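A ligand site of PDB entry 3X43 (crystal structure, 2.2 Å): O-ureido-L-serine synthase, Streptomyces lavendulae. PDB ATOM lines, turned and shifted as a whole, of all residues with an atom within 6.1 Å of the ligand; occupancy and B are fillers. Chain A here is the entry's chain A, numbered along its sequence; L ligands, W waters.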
ATOM      1  N   SER A  41       0.473   3.097  -2.417  1.00  0.00           N
ATOM      2  CA  SER A  41       0.557   3.530  -3.808  1.00  0.00           C
ATOM      3  C   SER A  41      -0.641   3.075  -4.644  1.00  0.00           C
ATOM      4  O   SER A  41      -1.527   2.384  -4.151  1.00  0.00           O
ATOM      5  CB  SER A  41       1.831   3.002  -4.462  1.00  0.00           C
ATOM      6  OG  SER A  41       1.657   1.679  -4.913  1.00  0.00           O
ATOM      7  N   VAL A  42      -0.648   3.479  -5.912  1.00  0.00           N
ATOM      8  CA  VAL A  42      -1.707   3.121  -6.849  1.00  0.00           C
ATOM      9  C   VAL A  42      -1.655   1.623  -7.183  1.00  0.00           C
ATOM     10  O   VAL A  42      -2.655   1.030  -7.599  1.00  0.00           O
ATOM     11  CB  VAL A  42      -1.580   3.987  -8.139  1.00  0.00           C
ATOM     12  CG1 VAL A  42      -0.277   3.679  -8.866  1.00  0.00           C
ATOM     13  CG2 VAL A  42      -2.758   3.750  -9.046  1.00  0.00           C
ATOM     14  N   LYS A  43      -0.499   0.992  -6.956  1.00  0.00           N
ATOM     15  CA  LYS A  43      -0.370  -0.437  -7.280  1.00  0.00           C
ATOM     16  C   LYS A  43      -1.341  -1.351  -6.538  1.00  0.00           C
ATOM     17  O   LYS A  43      -1.555  -2.494  -6.953  1.00  0.00           O
ATOM     18  CB  LYS A  43       1.071  -0.909  -7.038  1.00  0.00           C
ATOM     19  CG  LYS A  43       2.068  -0.418  -8.085  1.00  0.00           C
ATOM     20  CD  LYS A  43       1.565  -0.695  -9.488  1.00  0.00           C
ATOM     21  CE  LYS A  43       2.623  -0.368 -10.504  1.00  0.00           C
ATOM     22  NZ  LYS A  43       3.216   0.938 -10.177  1.00  0.00           N
ATOM     23  N   LEU A  46      -4.043  -2.641  -9.054  1.00  0.00           N
ATOM     24  CA  LEU A  46      -3.785  -3.779  -9.935  1.00  0.00           C
ATOM     25  C   LEU A  46      -3.514  -5.072  -9.170  1.00  0.00           C
ATOM     26  O   LEU A  46      -3.875  -6.151  -9.619  1.00  0.00           O
ATOM     27  CB  LEU A  46      -2.658  -3.445 -10.927  1.00  0.00           C
ATOM     28  CG  LEU A  46      -1.187  -3.717 -10.643  1.00  0.00           C
ATOM     29  CD1 LEU A  46      -0.867  -5.212 -10.700  1.00  0.00           C
ATOM     30  CD2 LEU A  46      -0.373  -2.986 -11.717  1.00  0.00           C
ATOM     31  N   SER A  71       9.590  -3.228  -9.426  1.00  0.00           N
ATOM     32  CA  SER A  71      10.492  -2.091  -9.260  1.00  0.00           C
ATOM     33  C   SER A  71      10.355  -1.638  -7.811  1.00  0.00           C
ATOM     34  O   SER A  71      11.125  -0.821  -7.323  1.00  0.00           O
ATOM     35  CB  SER A  71      10.082  -0.949 -10.191  1.00  0.00           C
ATOM     36  OG  SER A  71       8.692  -1.019 -10.519  1.00  0.00           O
ATOM     37  N   ASN A  73       6.891  -0.921  -5.865  1.00  0.00           N
ATOM     38  CA  ASN A  73       5.476  -0.831  -5.514  1.00  0.00           C
ATOM     39  C   ASN A  73       4.607  -2.058  -5.805  1.00  0.00           C
ATOM     40  O   ASN A  73       3.828  -2.497  -4.950  1.00  0.00           O
ATOM     41  CB  ASN A  73       4.870   0.419  -6.156  1.00  0.00           C
ATOM     42  CG  ASN A  73       5.282   1.681  -5.418  1.00  0.00           C
ATOM     43  OD1 ASN A  73       5.748   1.624  -4.282  1.00  0.00           O
ATOM     44  ND2 ASN A  73       5.111   2.824  -6.058  1.00  0.00           N
ATOM     45  N   VAL A  74       4.728  -2.617  -7.010  1.00  0.00           N
ATOM     46  CA  VAL A  74       3.960  -3.800  -7.356  1.00  0.00           C
ATOM     47  C   VAL A  74       4.271  -4.913  -6.350  1.00  0.00           C
ATOM     48  O   VAL A  74       3.370  -5.624  -5.902  1.00  0.00           O
ATOM     49  CB  VAL A  74       4.316  -4.304  -8.773  1.00  0.00           C
ATOM     50  CG1 VAL A  74       3.590  -5.600  -9.058  1.00  0.00           C
ATOM     51  CG2 VAL A  74       3.944  -3.247  -9.801  1.00  0.00           C
ATOM     52  N   ARG A 101      13.002  -0.842   0.039  1.00  0.00           N
ATOM     53  CA  ARG A 101      11.914  -1.361  -0.787  1.00  0.00           C
ATOM     54  C   ARG A 101      11.935  -2.863  -0.560  1.00  0.00           C
ATOM     55  O   ARG A 101      10.973  -3.564  -0.872  1.00  0.00           O
ATOM     56  CB  ARG A 101      12.157  -1.042  -2.261  1.00  0.00           C
ATOM     57  CG  ARG A 101      11.052  -0.221  -2.923  1.00  0.00           C
ATOM     58  CD  ARG A 101      11.626   0.924  -3.745  1.00  0.00           C
ATOM     59  NE  ARG A 101      10.648   1.452  -4.696  1.00  0.00           N
ATOM     60  CZ  ARG A 101      10.292   2.731  -4.779  1.00  0.00           C
ATOM     61  NH1 ARG A 101      10.835   3.620  -3.962  1.00  0.00           N
ATOM     62  NH2 ARG A 101       9.397   3.116  -5.671  1.00  0.00           N
ATOM     63  N   ASN A 148      -5.372  -5.153 -15.110  1.00  0.00           N
ATOM     64  CA  ASN A 148      -4.710  -3.931 -14.652  1.00  0.00           C
ATOM     65  C   ASN A 148      -5.467  -2.699 -15.135  1.00  0.00           C
ATOM     66  O   ASN A 148      -5.996  -1.937 -14.329  1.00  0.00           O
ATOM     67  CB  ASN A 148      -3.266  -3.949 -15.148  1.00  0.00           C
ATOM     68  CG  ASN A 148      -2.528  -2.669 -14.839  1.00  0.00           C
ATOM     69  OD1 ASN A 148      -3.085  -1.732 -14.277  1.00  0.00           O
ATOM     70  ND2 ASN A 148      -1.242  -2.620 -15.220  1.00  0.00           N
ATOM     71  N   HIS A 152      -8.818   0.232 -13.404  1.00  0.00           N
ATOM     72  CA  HIS A 152      -8.763   1.698 -13.446  1.00  0.00           C
ATOM     73  C   HIS A 152     -10.002   2.262 -14.129  1.00  0.00           C
ATOM     74  O   HIS A 152     -10.443   3.365 -13.803  1.00  0.00           O
ATOM     75  CB  HIS A 152      -7.497   2.180 -14.184  1.00  0.00           C
ATOM     76  CG  HIS A 152      -6.243   1.971 -13.402  1.00  0.00           C
ATOM     77  ND1 HIS A 152      -5.897   2.758 -12.320  1.00  0.00           N
ATOM     78  CD2 HIS A 152      -5.269   1.033 -13.513  1.00  0.00           C
ATOM     79  CE1 HIS A 152      -4.774   2.312 -11.790  1.00  0.00           C
ATOM     80  NE2 HIS A 152      -4.376   1.267 -12.494  1.00  0.00           N
ATOM     81  N   THR A 174      -0.693  12.348 -16.241  1.00  0.00           N
ATOM     82  CA  THR A 174      -0.192  11.131 -15.632  1.00  0.00           C
ATOM     83  C   THR A 174       0.998  10.538 -16.369  1.00  0.00           C
ATOM     84  O   THR A 174       1.086  10.616 -17.598  1.00  0.00           O
ATOM     85  CB  THR A 174      -1.293  10.051 -15.594  1.00  0.00           C
ATOM     86  OG1 THR A 174      -0.723   8.796 -15.207  1.00  0.00           O
ATOM     87  CG2 THR A 174      -1.919   9.900 -16.974  1.00  0.00           C
ATOM     88  N   GLY A 175       1.913   9.966 -15.610  1.00  0.00           N
ATOM     89  CA  GLY A 175       3.060   9.328 -16.228  1.00  0.00           C
ATOM     90  C   GLY A 175       2.603   7.902 -16.465  1.00  0.00           C
ATOM     91  O   GLY A 175       1.406   7.618 -16.356  1.00  0.00           O
ATOM     92  N   PHE A 176       3.513   6.988 -16.775  1.00  0.00           N
ATOM     93  CA  PHE A 176       3.102   5.616 -16.971  1.00  0.00           C
ATOM     94  C   PHE A 176       4.238   4.631 -16.777  1.00  0.00           C
ATOM     95  O   PHE A 176       5.405   4.937 -17.075  1.00  0.00           O
ATOM     96  CB  PHE A 176       2.474   5.432 -18.359  1.00  0.00           C
ATOM     97  CG  PHE A 176       3.440   5.624 -19.500  1.00  0.00           C
ATOM     98  CD1 PHE A 176       4.305   4.609 -19.870  1.00  0.00           C
ATOM     99  CD2 PHE A 176       3.464   6.831 -20.186  1.00  0.00           C
ATOM    100  CE1 PHE A 176       5.189   4.784 -20.921  1.00  0.00           C
ATOM    101  CE2 PHE A 176       4.353   7.023 -21.241  1.00  0.00           C
ATOM    102  CZ  PHE A 176       5.213   5.991 -21.607  1.00  0.00           C
ATOM    103  N   GLY A 177       3.879   3.475 -16.253  1.00  0.00           N
ATOM    104  CA  GLY A 177       4.830   2.407 -16.004  1.00  0.00           C
ATOM    105  C   GLY A 177       4.247   1.202 -16.704  1.00  0.00           C
ATOM    106  O   GLY A 177       4.789   0.750 -17.708  1.00  0.00           O
ATOM    107  N   THR A 178       3.136   0.701 -16.163  1.00  0.00           N
ATOM    108  CA  THR A 178       2.446  -0.436 -16.758  1.00  0.00           C
ATOM    109  C   THR A 178       1.493   0.138 -17.818  1.00  0.00           C
ATOM    110  O   THR A 178       1.124  -0.546 -18.757  1.00  0.00           O
ATOM    111  CB  THR A 178       1.598  -1.215 -15.712  1.00  0.00           C
ATOM    112  OG1 THR A 178       0.403  -0.470 -15.386  1.00  0.00           O
ATOM    113  CG2 THR A 178       2.418  -1.465 -14.441  1.00  0.00           C
ATOM    114  N   THR A 179       1.130   1.402 -17.626  1.00  0.00           N
ATOM    115  CA  THR A 179       0.216   2.166 -18.476  1.00  0.00           C
ATOM    116  C   THR A 179      -1.258   1.858 -18.157  1.00  0.00           C
ATOM    117  O   THR A 179      -2.171   2.264 -18.911  1.00  0.00           O
ATOM    118  CB  THR A 179       0.480   1.951 -20.018  1.00  0.00           C
ATOM    119  OG1 THR A 179       0.014   0.656 -20.434  1.00  0.00           O
ATOM    120  CG2 THR A 179       1.958   2.078 -20.344  1.00  0.00           C
ATOM    121  N   GLY A 180      -1.481   1.158 -17.047  1.00  0.00           N
ATOM    122  CA  GLY A 180      -2.825   0.809 -16.645  1.00  0.00           C
ATOM    123  C   GLY A 180      -3.690   2.015 -16.330  1.00  0.00           C
ATOM    124  O   GLY A 180      -4.842   2.102 -16.752  1.00  0.00           O
ATOM    125  N   THR A 181      -3.139   2.957 -15.584  1.00  0.00           N
ATOM    126  CA  THR A 181      -3.863   4.168 -15.212  1.00  0.00           C
ATOM    127  C   THR A 181      -4.216   4.990 -16.444  1.00  0.00           C
ATOM    128  O   THR A 181      -5.377   5.337 -16.677  1.00  0.00           O
ATOM    129  CB  THR A 181      -3.012   5.010 -14.246  1.00  0.00           C
ATOM    130  OG1 THR A 181      -2.673   4.200 -13.102  1.00  0.00           O
ATOM    131  CG2 THR A 181      -3.751   6.258 -13.792  1.00  0.00           C
ATOM    132  N   LEU A 182      -3.194   5.282 -17.249  1.00  0.00           N
ATOM    133  CA  LEU A 182      -3.349   6.054 -18.488  1.00  0.00           C
ATOM    134  C   LEU A 182      -4.380   5.427 -19.411  1.00  0.00           C
ATOM    135  O   LEU A 182      -5.271   6.116 -19.898  1.00  0.00           O
ATOM    136  CB  LEU A 182      -1.999   6.128 -19.214  1.00  0.00           C
ATOM    137  CG  LEU A 182      -2.006   6.624 -20.676  1.00  0.00           C
ATOM    138  CD1 LEU A 182      -2.761   7.941 -20.796  1.00  0.00           C
ATOM    139  CD2 LEU A 182      -0.573   6.780 -21.154  1.00  0.00           C
ATOM    140  N   GLN A 220      11.270   6.808 -10.464  1.00  0.00           N
ATOM    141  CA  GLN A 220      10.755   5.487 -10.106  1.00  0.00           C
ATOM    142  C   GLN A 220       9.284   5.256 -10.454  1.00  0.00           C
ATOM    143  O   GLN A 220       8.431   6.135 -10.271  1.00  0.00           O
ATOM    144  CB  GLN A 220      10.968   5.239  -8.612  1.00  0.00           C
ATOM    145  CG  GLN A 220      12.434   5.264  -8.206  1.00  0.00           C
ATOM    146  CD  GLN A 220      12.780   4.190  -7.177  1.00  0.00           C
ATOM    147  OE1 GLN A 220      13.583   4.419  -6.273  1.00  0.00           O
ATOM    148  NE2 GLN A 220      12.176   3.012  -7.324  1.00  0.00           N
ATOM    149  N   GLY A 221       9.003   4.062 -10.951  1.00  0.00           N
ATOM    150  CA  GLY A 221       7.647   3.715 -11.338  1.00  0.00           C
ATOM    151  C   GLY A 221       7.389   3.959 -12.801  1.00  0.00           C
ATOM    152  O   GLY A 221       6.592   3.247 -13.438  1.00  0.00           O
ATOM    153  N   LEU A 222       8.069   4.960 -13.369  1.00  0.00           N
ATOM    154  CA  LEU A 222       7.896   5.312 -14.774  1.00  0.00           C
ATOM    155  C   LEU A 222       8.798   4.608 -15.799  1.00  0.00           C
ATOM    156  O   LEU A 222       9.827   4.015 -15.464  1.00  0.00           O
ATOM    157  CB  LEU A 222       8.044   6.829 -14.951  1.00  0.00           C
ATOM    158  CG  LEU A 222       7.116   7.740 -14.162  1.00  0.00           C
ATOM    159  CD1 LEU A 222       7.228   9.155 -14.686  1.00  0.00           C
ATOM    160  CD2 LEU A 222       5.678   7.251 -14.272  1.00  0.00           C
ATOM    161  N   SER A 265       7.543  10.424  -9.238  1.00  0.00           N
ATOM    162  CA  SER A 265       6.697  10.427 -10.417  1.00  0.00           C
ATOM    163  C   SER A 265       5.551  11.411 -10.185  1.00  0.00           C
ATOM    164  O   SER A 265       5.054  12.025 -11.130  1.00  0.00           O
ATOM    165  CB  SER A 265       6.134   9.024 -10.707  1.00  0.00           C
ATOM    166  OG  SER A 265       5.364   8.522  -9.628  1.00  0.00           O
ATOM    167  N   ALA A 266       5.158  11.590  -8.929  1.00  0.00           N
ATOM    168  CA  ALA A 266       4.103  12.519  -8.569  1.00  0.00           C
ATOM    169  C   ALA A 266       4.631  13.933  -8.744  1.00  0.00           C
ATOM    170  O   ALA A 266       3.875  14.848  -9.066  1.00  0.00           O
ATOM    171  CB  ALA A 266       3.671  12.293  -7.128  1.00  0.00           C
ATOM    172  N   PRO A 291       1.042   8.937  -7.765  1.00  0.00           N
ATOM    173  CA  PRO A 291       1.262   7.494  -7.575  1.00  0.00           C
ATOM    174  C   PRO A 291       1.528   6.945  -6.188  1.00  0.00           C
ATOM    175  O   PRO A 291       0.936   5.934  -5.809  1.00  0.00           O
ATOM    176  CB  PRO A 291       2.379   7.180  -8.555  1.00  0.00           C
ATOM    177  CG  PRO A 291       2.175   8.207  -9.642  1.00  0.00           C
ATOM    178  CD  PRO A 291       1.829   9.452  -8.893  1.00  0.00           C
ATOM    179  N   ASP A 292       2.386   7.572  -5.406  1.00  0.00           N
ATOM    180  CA  ASP A 292       2.652   7.004  -4.095  1.00  0.00           C
ATOM    181  C   ASP A 292       3.110   7.967  -3.024  1.00  0.00           C
ATOM    182  O   ASP A 292       3.199   9.177  -3.238  1.00  0.00           O
ATOM    183  CB  ASP A 292       3.661   5.856  -4.219  1.00  0.00           C
ATOM    184  CG  ASP A 292       5.023   6.301  -4.732  1.00  0.00           C
ATOM    185  OD1 ASP A 292       5.242   7.522  -4.882  1.00  0.00           O
ATOM    186  OD2 ASP A 292       5.867   5.432  -4.982  1.00  0.00           O
ATOM    187  N   TYR A 297      10.955   7.198  -0.153  1.00  0.00           N
ATOM    188  CA  TYR A 297      11.995   7.774  -0.983  1.00  0.00           C
ATOM    189  C   TYR A 297      13.129   8.437  -0.172  1.00  0.00           C
ATOM    190  O   TYR A 297      13.997   9.095  -0.743  1.00  0.00           O
ATOM    191  CB  TYR A 297      11.371   8.786  -1.954  1.00  0.00           C
ATOM    192  CG  TYR A 297      10.492   8.128  -3.005  1.00  0.00           C
ATOM    193  CD1 TYR A 297      11.007   7.780  -4.260  1.00  0.00           C
ATOM    194  CD2 TYR A 297       9.160   7.820  -2.724  1.00  0.00           C
ATOM    195  CE1 TYR A 297      10.202   7.134  -5.209  1.00  0.00           C
ATOM    196  CE2 TYR A 297       8.358   7.176  -3.659  1.00  0.00           C
ATOM    197  CZ  TYR A 297       8.878   6.826  -4.892  1.00  0.00           C
ATOM    198  OH  TYR A 297       8.067   6.169  -5.794  1.00  0.00           O
HETATM  199  N1  LIG L   1       4.583   5.993 -10.512  1.00  0.00           N
HETATM  200  C1  LIG L   1       4.839   5.033  -9.521  1.00  0.00           C
HETATM  201  C2  LIG L   1       5.618   5.380  -8.272  1.00  0.00           C
HETATM  202  C3  LIG L   1       4.333   3.776  -9.727  1.00  0.00           C
HETATM  203  O1  LIG L   1       4.509   2.823  -8.797  1.00  0.00           O
HETATM  204  C4  LIG L   1       3.613   3.499 -10.904  1.00  0.00           C
HETATM  205  C5  LIG L   1       3.023   2.046 -11.150  1.00  0.00           C
HETATM  206  C6  LIG L   1       3.403   4.534 -11.867  1.00  0.00           C
HETATM  207  C7  LIG L   1       3.888   5.741 -11.634  1.00  0.00           C
HETATM  208  C8  LIG L   1       2.726   4.322 -13.227  1.00  0.00           C
HETATM  209  O2  LIG L   1       1.384   3.815 -13.136  1.00  0.00           O
HETATM  210  P1  LIG L   1       0.785   2.733 -14.145  1.00  0.00           P
HETATM  211  O3  LIG L   1       1.100   3.219 -15.489  1.00  0.00           O
HETATM  212  O4  LIG L   1      -0.667   2.655 -13.914  1.00  0.00           O
HETATM  213  O5  LIG L   1       1.440   1.451 -13.891  1.00  0.00           O
HETATM  214  O   HOH W   1      -0.362   5.161 -16.326  1.00  0.00           O
HETATM  215  O   HOH W   2      -1.758   0.058 -12.744  1.00  0.00           O
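N of Thr 178 sits at hydrogen-bond distance from O5 of the ligand (2.9 Å).
An oxygen (O3) of the ligand lies within hydrogen-bond range of the backbone NH (N) of Thr 179 (2.8 Å).
OG1 of Thr 178 is in hydrogen-bond range of O5 of the ligand.
The side-chain amide nitrogen of Asn 73 is in hydrogen-bond range of an oxygen (O1) of the ligand (2.8 Å).
The backbone NH (N) of Thr 181 sits at hydrogen-bond distance from an oxygen (O4) of the ligand (3.0 Å).
An oxygen (O4) of the ligand lies within hydrogen-bond range of the side-chain hydroxyl (OG1) of Thr 181 (2.7 Å).
A carbon (C5) of the ligand is bonded to the side-chain amino group (NZ) of Lys 43, 1.5 Å away.
O3 of the ligand lies within hydrogen-bond range of N of Gly 177, at 2.9 Å.
OG of Ser 265 is in hydrogen-bond range of N1 of the ligand (2.8 Å).
ND2 of Asn 73 lies within hydrogen-bond range of OD2 of Asp 292 (2.9 Å).
OG1 of Thr 178 lies within hydrogen-bond range of N of Gly 180 (3.0 Å).
O of Pro 291 sits at hydrogen-bond distance from N of Val 42, at 2.9 Å.
OH of Tyr 297 is in hydrogen-bond range of OD2 of Asp 292.
The side-chain amide nitrogen (NE2) of Gln 220 sits close to the guanidinium group (NH2) of Arg 101.
The side-chain hydroxyl (OH) of Tyr 297 is in hydrogen-bond range of the guanidinium group (NH2) of Arg 101, 3.3 Å away.
The backbone NH (N) of Lys 43 lies within hydrogen-bond range of the side-chain hydroxyl (OG) of Ser 41, 3.0 Å away.
The side-chain hydroxyl of Thr 181 sits close to a ring nitrogen (NE2) of His 152 (3.4 Å).
Merely in contact with the ligand: Phe 176 (3.5 Å), Gly 180 (3.6 Å), Gln 220 (3.5 Å), Gly 221 (3.6 Å), Leu 222 (3.5 Å), Pro 291 (3.2 Å), Asp 292 (3.3 Å) and Tyr 297 (3.6 Å).
Hydrophobic or aromatic side chains within 4 Å of the ligand: Phe 176, Leu 222 and Pro 291.
15 residues have an atom within 4 Å of the ligand: Lys 43, Asn 73, Phe 176, Gly 177, Thr 178, Thr 179, Gly 180, Thr 181, Gln 220, Gly 221, Leu 222, Ser 265, Pro 291, Asp 292 and Tyr 297.
The nearest printed residue that does not touch the ligand is His 152 (4.2 Å).
Water W1 lies within hydrogen-bond range of an oxygen (O3) of the ligand (2.6 Å), the backbone NH of Leu 182 (3.0 Å) and the backbone carbonyl oxygen of Gly 175 (3.0 Å).
Water W2 lies within hydrogen-bond range of the side-chain amide oxygen (OD1) of Asn 148 (2.7 Å), a ring nitrogen (NE2) of His 152 (2.9 Å), an oxygen (O4) of the ligand (3.1 Å) and the side-chain hydroxyl (OG1) of Thr 178 (3.5 Å).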
